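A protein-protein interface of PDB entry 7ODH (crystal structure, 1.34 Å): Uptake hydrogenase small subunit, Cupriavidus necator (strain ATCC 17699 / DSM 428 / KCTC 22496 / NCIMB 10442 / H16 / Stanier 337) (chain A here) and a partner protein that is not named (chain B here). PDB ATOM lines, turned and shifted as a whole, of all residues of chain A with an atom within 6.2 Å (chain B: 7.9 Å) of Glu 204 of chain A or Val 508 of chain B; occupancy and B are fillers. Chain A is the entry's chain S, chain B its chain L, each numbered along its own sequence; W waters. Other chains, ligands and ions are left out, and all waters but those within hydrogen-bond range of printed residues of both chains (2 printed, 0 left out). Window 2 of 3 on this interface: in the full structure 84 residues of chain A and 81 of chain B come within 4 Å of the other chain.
The backbone NH (N) of Thr 505 of chain B lies within hydrogen-bond range of the side-chain carboxylate (OD2) of Asp 206 of chain A (2.9 Å).
N of Glu 204 of chain A sits at hydrogen-bond distance from OD2 of Asp 207 of chain A (3.0 Å).
Among the printed residues, pairs that only touch across the chains: Trp 205 of chain A with Trp 511 of chain B (3.4 Å), Trp 205 of chain A with Val 508 of chain B (3.4 Å), Trp 205 of chain A with Leu 233 of chain B (3.5 Å), Asp 206 of chain A with Ala 506 of chain B (3.6 Å), Glu 204 of chain A with Val 508 of chain B (3.7 Å) and Trp 205 of chain A with Ala 506 of chain B (3.9 Å).
Val 508 of chain B touches just these residues of chain A: Glu 204 and Trp 205. Printed residues of chain A within 4 Å of Trp 511 of chain B: Trp 205 (3.4 Å). Printed residues of chain A within 4 Å of Leu 233 of chain B: Trp 205. Printed residues of chain B within 4 Å of Trp 205 of chain A: Leu 233 (3.5 Å), Ala 506 (3.9 Å), Val 508 (3.4 Å) and Trp 511 (3.4 Å). Glu 208 of chain A touches none of the printed residues of chain B. The nearest printed residue of chain A that does not touch Trp 511 of chain B is Met 219 of chain A (4.8 Å).
Hydrophobic or aromatic side chains of chain A within 4 Å of the printed part of chain B: Trp 205. Hydrophobic or aromatic side chains of chain B within 4 Å of the printed part of chain A: Leu 233, Ala 506, Val 508 and Trp 511. Among the printed residues, 7 pairs touch across the chains. Among the printed residues, no Asp or Glu carboxylate lies within 4 Å of a Lys or Arg side-chain nitrogen of the other chain.
Water W2 bridges OD1 of Asp 206 of chain A (2.6 Å) and OG1 of Thr 505 of chain B (2.8 Å). Water W1 lies within hydrogen-bond range of OD2 of Asp 206 of chain A (2.6 Å) and O of Ala 506 of chain B (2.8 Å).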
ATOM      1  N   VAL A 202      -8.051  14.189  25.982  1.00  0.00           N
ATOM      2  CA  VAL A 202      -6.621  14.466  25.679  1.00  0.00           C
ATOM      3  C   VAL A 202      -6.058  13.276  24.893  1.00  0.00           C
ATOM      4  O   VAL A 202      -6.300  12.128  25.297  1.00  0.00           O
ATOM      5  CB  VAL A 202      -5.828  14.714  26.971  1.00  0.00           C
ATOM      6  CG1 VAL A 202      -4.355  14.967  26.683  1.00  0.00           C
ATOM      7  CG2 VAL A 202      -6.434  15.851  27.781  1.00  0.00           C
ATOM      8  N   GLU A 203      -5.320  13.531  23.812  1.00  0.00           N
ATOM      9  CA  GLU A 203      -4.665  12.456  23.014  1.00  0.00           C
ATOM     10  C   GLU A 203      -3.136  12.567  23.108  1.00  0.00           C
ATOM     11  O   GLU A 203      -2.468  11.532  22.954  1.00  0.00           O
ATOM     12  CB  GLU A 203      -5.148  12.490  21.562  1.00  0.00           C
ATOM     13  CG  GLU A 203      -6.593  12.010  21.370  1.00  0.00           C
ATOM     14  CD  GLU A 203      -6.808  10.510  21.179  1.00  0.00           C
ATOM     15  OE1 GLU A 203      -5.982   9.714  21.700  1.00  0.00           O
ATOM     16  OE2 GLU A 203      -7.826  10.131  20.525  1.00  0.00           O
ATOM     17  N   GLU A 204      -2.595  13.772  23.309  1.00  0.00           N
ATOM     18  CA  GLU A 204      -1.141  14.017  23.473  1.00  0.00           C
ATOM     19  C   GLU A 204      -0.962  15.062  24.567  1.00  0.00           C
ATOM     20  O   GLU A 204      -1.811  15.968  24.678  1.00  0.00           O
ATOM     21  CB  GLU A 204      -0.486  14.506  22.176  1.00  0.00           C
ATOM     22  CG  GLU A 204      -0.562  13.500  21.040  1.00  0.00           C
ATOM     23  CD  GLU A 204       0.088  13.934  19.738  1.00  0.00           C
ATOM     24  OE1 GLU A 204       0.754  14.985  19.729  1.00  0.00           O
ATOM     25  OE2 GLU A 204      -0.086  13.226  18.729  1.00  0.00           O
ATOM     26  N   TRP A 205       0.083  14.942  25.371  1.00  0.00           N
ATOM     27  CA  TRP A 205       0.313  15.945  26.435  1.00  0.00           C
ATOM     28  C   TRP A 205       0.318  17.347  25.816  1.00  0.00           C
ATOM     29  O   TRP A 205       0.975  17.582  24.711  1.00  0.00           O
ATOM     30  CB  TRP A 205       1.588  15.642  27.222  1.00  0.00           C
ATOM     31  CG  TRP A 205       1.549  14.279  27.831  1.00  0.00           C
ATOM     32  CD1 TRP A 205       2.299  13.201  27.465  1.00  0.00           C
ATOM     33  CD2 TRP A 205       0.670  13.825  28.877  1.00  0.00           C
ATOM     34  NE1 TRP A 205       1.949  12.112  28.210  1.00  0.00           N
ATOM     35  CE2 TRP A 205       0.962  12.461  29.090  1.00  0.00           C
ATOM     36  CE3 TRP A 205      -0.323  14.429  29.656  1.00  0.00           C
ATOM     37  CZ2 TRP A 205       0.302  11.701  30.051  1.00  0.00           C
ATOM     38  CZ3 TRP A 205      -0.978  13.674  30.603  1.00  0.00           C
ATOM     39  CH2 TRP A 205      -0.661  12.330  30.803  1.00  0.00           C
ATOM     40  N   ASP A 206      -0.305  18.281  26.526  1.00  0.00           N
ATOM     41  CA  ASP A 206      -0.302  19.727  26.198  1.00  0.00           C
ATOM     42  C   ASP A 206      -0.919  19.970  24.819  1.00  0.00           C
ATOM     43  O   ASP A 206      -0.633  21.027  24.223  1.00  0.00           O
ATOM     44  CB  ASP A 206       1.112  20.307  26.257  1.00  0.00           C
ATOM     45  CG  ASP A 206       1.105  21.816  26.382  1.00  0.00           C
ATOM     46  OD1 ASP A 206       0.078  22.350  26.850  1.00  0.00           O
ATOM     47  OD2 ASP A 206       2.114  22.441  25.997  1.00  0.00           O
ATOM     48  N   ASP A 207      -1.796  19.081  24.357  1.00  0.00           N
ATOM     49  CA  ASP A 207      -2.616  19.359  23.154  1.00  0.00           C
ATOM     50  C   ASP A 207      -3.716  20.356  23.547  1.00  0.00           C
ATOM     51  O   ASP A 207      -3.824  20.723  24.731  1.00  0.00           O
ATOM     52  CB  ASP A 207      -3.094  18.070  22.483  1.00  0.00           C
ATOM     53  CG  ASP A 207      -4.100  17.234  23.249  1.00  0.00           C
ATOM     54  OD1 ASP A 207      -4.576  17.696  24.311  1.00  0.00           O
ATOM     55  OD2 ASP A 207      -4.392  16.107  22.769  1.00  0.00           O
ATOM     56  N   GLU A 208      -4.473  20.844  22.571  1.00  0.00           N
ATOM     57  CA  GLU A 208      -5.531  21.850  22.837  1.00  0.00           C
ATOM     58  C   GLU A 208      -6.510  21.261  23.860  1.00  0.00           C
ATOM     59  O   GLU A 208      -6.958  21.997  24.749  1.00  0.00           O
ATOM     60  CB  GLU A 208      -6.242  22.256  21.546  1.00  0.00           C
ATOM     61  CG  GLU A 208      -5.370  23.051  20.589  1.00  0.00           C
ATOM     62  CD  GLU A 208      -4.777  24.332  21.156  1.00  0.00           C
ATOM     63  OE1 GLU A 208      -5.372  24.894  22.099  1.00  0.00           O
ATOM     64  OE2 GLU A 208      -3.714  24.762  20.654  1.00  0.00           O
ATOM     65  N   ALA A 210      -5.905  19.101  26.309  1.00  0.00           N
ATOM     66  CA  ALA A 210      -5.277  19.156  27.650  1.00  0.00           C
ATOM     67  C   ALA A 210      -5.452  20.562  28.245  1.00  0.00           C
ATOM     68  O   ALA A 210      -5.743  20.685  29.445  1.00  0.00           O
ATOM     69  CB  ALA A 210      -3.822  18.776  27.557  1.00  0.00           C
ATOM     70  N   MET A 219      -5.098   8.953  28.013  1.00  0.00           N
ATOM     71  CA  MET A 219      -3.715   9.106  28.531  1.00  0.00           C
ATOM     72  C   MET A 219      -3.464   8.111  29.675  1.00  0.00           C
ATOM     73  O   MET A 219      -2.410   8.202  30.307  1.00  0.00           O
ATOM     74  CB  MET A 219      -3.462  10.542  29.000  1.00  0.00           C
ATOM     75  CG  MET A 219      -3.751  11.596  27.940  1.00  0.00           C
ATOM     76  SD  MET A 219      -3.003  11.267  26.313  1.00  0.00           S
ATOM     77  CE  MET A 219      -1.256  11.348  26.708  1.00  0.00           C
ATOM     78  N   ILE B  96      15.630  14.401  24.636  1.00  0.00           N
ATOM     79  CA  ILE B  96      14.406  15.240  24.770  1.00  0.00           C
ATOM     80  C   ILE B  96      14.788  16.520  25.515  1.00  0.00           C
ATOM     81  O   ILE B  96      15.309  16.407  26.635  1.00  0.00           O
ATOM     82  CB  ILE B  96      13.301  14.463  25.504  1.00  0.00           C
ATOM     83  CG1 ILE B  96      12.919  13.193  24.737  1.00  0.00           C
ATOM     84  CG2 ILE B  96      12.096  15.351  25.774  1.00  0.00           C
ATOM     85  CD1 ILE B  96      12.076  12.217  25.518  1.00  0.00           C
ATOM     86  N   ARG B  97      14.510  17.687  24.934  1.00  0.00           N
ATOM     87  CA  ARG B  97      14.636  18.988  25.635  1.00  0.00           C
ATOM     88  C   ARG B  97      13.236  19.455  26.033  1.00  0.00           C
ATOM     89  O   ARG B  97      12.366  19.568  25.154  1.00  0.00           O
ATOM     90  CB  ARG B  97      15.367  20.016  24.763  1.00  0.00           C
ATOM     91  CG  ARG B  97      16.811  19.644  24.443  1.00  0.00           C
ATOM     92  CD  ARG B  97      17.681  19.488  25.680  1.00  0.00           C
ATOM     93  NE  ARG B  97      19.098  19.304  25.382  1.00  0.00           N
ATOM     94  CZ  ARG B  97      19.988  20.286  25.216  1.00  0.00           C
ATOM     95  NH1 ARG B  97      19.623  21.556  25.301  1.00  0.00           N
ATOM     96  NH2 ARG B  97      21.248  19.988  24.955  1.00  0.00           N
ATOM     97  N   PRO B  99      10.303  22.134  27.498  1.00  0.00           N
ATOM     98  CA  PRO B  99      10.076  23.564  27.331  1.00  0.00           C
ATOM     99  C   PRO B  99      10.384  24.359  28.607  1.00  0.00           C
ATOM    100  O   PRO B  99      10.402  23.803  29.703  1.00  0.00           O
ATOM    101  CB  PRO B  99       8.596  23.685  26.961  1.00  0.00           C
ATOM    102  CG  PRO B  99       7.962  22.376  27.348  1.00  0.00           C
ATOM    103  CD  PRO B  99       9.067  21.344  27.427  1.00  0.00           C
ATOM    104  N   LEU B 233       6.403  13.922  34.506  1.00  0.00           N
ATOM    105  CA  LEU B 233       6.125  13.531  33.110  1.00  0.00           C
ATOM    106  C   LEU B 233       7.413  13.564  32.302  1.00  0.00           C
ATOM    107  O   LEU B 233       8.089  14.601  32.292  1.00  0.00           O
ATOM    108  CB  LEU B 233       5.105  14.505  32.528  1.00  0.00           C
ATOM    109  CG  LEU B 233       4.618  14.171  31.125  1.00  0.00           C
ATOM    110  CD1 LEU B 233       3.739  12.931  31.145  1.00  0.00           C
ATOM    111  CD2 LEU B 233       3.882  15.354  30.521  1.00  0.00           C
ATOM    112  N   VAL B 234       7.693  12.496  31.573  1.00  0.00           N
ATOM    113  CA  VAL B 234       8.800  12.517  30.583  1.00  0.00           C
ATOM    114  C   VAL B 234       8.419  13.491  29.468  1.00  0.00           C
ATOM    115  O   VAL B 234       7.364  13.295  28.830  1.00  0.00           O
ATOM    116  CB  VAL B 234       9.112  11.119  30.034  1.00  0.00           C
ATOM    117  CG1 VAL B 234      10.105  11.191  28.886  1.00  0.00           C
ATOM    118  CG2 VAL B 234       9.627  10.208  31.132  1.00  0.00           C
ATOM    119  N   GLY B 235       9.225  14.535  29.290  1.00  0.00           N
ATOM    120  CA  GLY B 235       9.021  15.535  28.231  1.00  0.00           C
ATOM    121  C   GLY B 235       8.496  16.863  28.750  1.00  0.00           C
ATOM    122  O   GLY B 235       8.446  17.814  27.960  1.00  0.00           O
ATOM    123  N   GLY B 236       8.123  16.967  30.022  1.00  0.00           N
ATOM    124  CA  GLY B 236       7.681  18.263  30.563  1.00  0.00           C
ATOM    125  C   GLY B 236       6.920  18.107  31.855  1.00  0.00           C
ATOM    126  O   GLY B 236       7.395  17.389  32.750  1.00  0.00           O
ATOM    127  N   THR B 505       4.063  23.377  27.885  1.00  0.00           N
ATOM    128  CA  THR B 505       4.447  22.624  29.109  1.00  0.00           C
ATOM    129  C   THR B 505       4.995  21.227  28.797  1.00  0.00           C
ATOM    130  O   THR B 505       5.565  20.626  29.714  1.00  0.00           O
ATOM    131  CB  THR B 505       3.286  22.496  30.107  1.00  0.00           C
ATOM    132  OG1 THR B 505       2.088  22.089  29.439  1.00  0.00           O
ATOM    133  CG2 THR B 505       3.027  23.780  30.864  1.00  0.00           C
ATOM    134  N   ALA B 506       4.862  20.705  27.583  1.00  0.00           N
ATOM    135  CA  ALA B 506       5.393  19.358  27.275  1.00  0.00           C
ATOM    136  C   ALA B 506       5.876  19.280  25.830  1.00  0.00           C
ATOM    137  O   ALA B 506       5.204  19.813  24.928  1.00  0.00           O
ATOM    138  CB  ALA B 506       4.355  18.307  27.571  1.00  0.00           C
ATOM    139  N   ASN B 507       7.021  18.632  25.651  1.00  0.00           N
ATOM    140  CA  ASN B 507       7.569  18.219  24.341  1.00  0.00           C
ATOM    141  C   ASN B 507       7.186  16.753  24.149  1.00  0.00           C
ATOM    142  O   ASN B 507       7.668  15.922  24.933  1.00  0.00           O
ATOM    143  CB  ASN B 507       9.079  18.452  24.293  1.00  0.00           C
ATOM    144  CG  ASN B 507       9.729  17.941  23.028  1.00  0.00           C
ATOM    145  OD1 ASN B 507       9.074  17.343  22.177  1.00  0.00           O
ATOM    146  ND2 ASN B 507      11.030  18.151  22.914  1.00  0.00           N
ATOM    147  N   VAL B 508       6.313  16.462  23.186  1.00  0.00           N
ATOM    148  CA  VAL B 508       5.779  15.087  22.954  1.00  0.00           C
ATOM    149  C   VAL B 508       6.391  14.487  21.683  1.00  0.00           C
ATOM    150  O   VAL B 508       5.936  13.406  21.269  1.00  0.00           O
ATOM    151  CB  VAL B 508       4.242  15.087  22.883  1.00  0.00           C
ATOM    152  CG1 VAL B 508       3.630  15.557  24.190  1.00  0.00           C
ATOM    153  CG2 VAL B 508       3.721  15.913  21.716  1.00  0.00           C
ATOM    154  N   ASP B 509       7.398  15.134  21.096  1.00  0.00           N
ATOM    155  CA  ASP B 509       7.987  14.689  19.805  1.00  0.00           C
ATOM    156  C   ASP B 509       8.449  13.232  19.928  1.00  0.00           C
ATOM    157  O   ASP B 509       8.306  12.484  18.947  1.00  0.00           O
ATOM    158  CB  ASP B 509       9.144  15.590  19.368  1.00  0.00           C
ATOM    159  CG  ASP B 509       8.701  16.971  18.922  1.00  0.00           C
ATOM    160  OD1 ASP B 509       7.474  17.183  18.798  1.00  0.00           O
ATOM    161  OD2 ASP B 509       9.584  17.825  18.708  1.00  0.00           O
ATOM    162  N   LYS B 510       8.991  12.853  21.087  1.00  0.00           N
ATOM    163  CA  LYS B 510       9.561  11.500  21.318  1.00  0.00           C
ATOM    164  C   LYS B 510       8.795  10.789  22.437  1.00  0.00           C
ATOM    165  O   LYS B 510       9.371   9.903  23.075  1.00  0.00           O
ATOM    166  CB  LYS B 510      11.057  11.606  21.618  1.00  0.00           C
ATOM    167  CG  LYS B 510      11.881  12.151  20.461  1.00  0.00           C
ATOM    168  CD  LYS B 510      13.308  12.475  20.810  1.00  0.00           C
ATOM    169  CE  LYS B 510      13.948  13.385  19.783  1.00  0.00           C
ATOM    170  NZ  LYS B 510      15.349  13.710  20.133  1.00  0.00           N
ATOM    171  N   TRP B 511       7.518  11.110  22.628  1.00  0.00           N
ATOM    172  CA  TRP B 511       6.663  10.383  23.599  1.00  0.00           C
ATOM    173  C   TRP B 511       6.498   8.924  23.155  1.00  0.00           C
ATOM    174  O   TRP B 511       6.592   8.025  23.999  1.00  0.00           O
ATOM    175  CB  TRP B 511       5.312  11.082  23.762  1.00  0.00           C
ATOM    176  CG  TRP B 511       4.374  10.314  24.635  1.00  0.00           C
ATOM    177  CD1 TRP B 511       3.314   9.559  24.234  1.00  0.00           C
ATOM    178  CD2 TRP B 511       4.458  10.166  26.065  1.00  0.00           C
ATOM    179  NE1 TRP B 511       2.708   8.985  25.319  1.00  0.00           N
ATOM    180  CE2 TRP B 511       3.381   9.347  26.457  1.00  0.00           C
ATOM    181  CE3 TRP B 511       5.303  10.687  27.052  1.00  0.00           C
ATOM    182  CZ2 TRP B 511       3.169   8.990  27.788  1.00  0.00           C
ATOM    183  CZ3 TRP B 511       5.077  10.352  28.368  1.00  0.00           C
ATOM    184  CH2 TRP B 511       4.020   9.517  28.730  1.00  0.00           C
ATOM    185  N   ASP B 512       6.231   8.694  21.874  1.00  0.00           N
ATOM    186  CA  ASP B 512       5.914   7.337  21.360  1.00  0.00           C
ATOM    187  C   ASP B 512       7.215   6.564  21.190  1.00  0.00           C
ATOM    188  O   ASP B 512       8.122   7.039  20.519  1.00  0.00           O
ATOM    189  CB  ASP B 512       5.141   7.413  20.044  1.00  0.00           C
ATOM    190  CG  ASP B 512       4.562   6.081  19.611  1.00  0.00           C
ATOM    191  OD1 ASP B 512       5.334   5.119  19.497  1.00  0.00           O
ATOM    192  OD2 ASP B 512       3.338   6.006  19.437  1.00  0.00           O
ATOM    193  N   THR B 515       9.534   6.194  18.041  1.00  0.00           N
ATOM    194  CA  THR B 515      10.464   7.291  17.661  1.00  0.00           C
ATOM    195  C   THR B 515      11.841   7.084  18.297  1.00  0.00           C
ATOM    196  O   THR B 515      12.763   7.836  17.943  1.00  0.00           O
ATOM    197  CB  THR B 515       9.933   8.674  18.062  1.00  0.00           C
ATOM    198  OG1 THR B 515       9.899   8.765  19.488  1.00  0.00           O
ATOM    199  CG2 THR B 515       8.571   8.975  17.477  1.00  0.00           C
ATOM    200  N   TRP B 516      11.977   6.144  19.234  1.00  0.00           N
ATOM    201  CA  TRP B 516      13.200   6.033  20.070  1.00  0.00           C
ATOM    202  C   TRP B 516      14.303   5.337  19.290  1.00  0.00           C
ATOM    203  O   TRP B 516      14.038   4.473  18.461  1.00  0.00           O
ATOM    204  CB  TRP B 516      12.940   5.299  21.387  1.00  0.00           C
ATOM    205  CG  TRP B 516      11.934   5.948  22.282  1.00  0.00           C
ATOM    206  CD1 TRP B 516      11.288   7.138  22.106  1.00  0.00           C
ATOM    207  CD2 TRP B 516      11.450   5.408  23.520  1.00  0.00           C
ATOM    208  NE1 TRP B 516      10.418   7.360  23.144  1.00  0.00           N
ATOM    209  CE2 TRP B 516      10.505   6.320  24.030  1.00  0.00           C
ATOM    210  CE3 TRP B 516      11.717   4.240  24.238  1.00  0.00           C
ATOM    211  CZ2 TRP B 516       9.821   6.090  25.224  1.00  0.00           C
ATOM    212  CZ3 TRP B 516      11.045   4.018  25.420  1.00  0.00           C
ATOM    213  CH2 TRP B 516      10.112   4.933  25.906  1.00  0.00           C
HETATM  214  O   HOH W   1       3.658  21.938  23.946  1.00  0.00           O
HETATM  215  O   HOH W   2       0.492  24.216  28.605  1.00  0.00           O
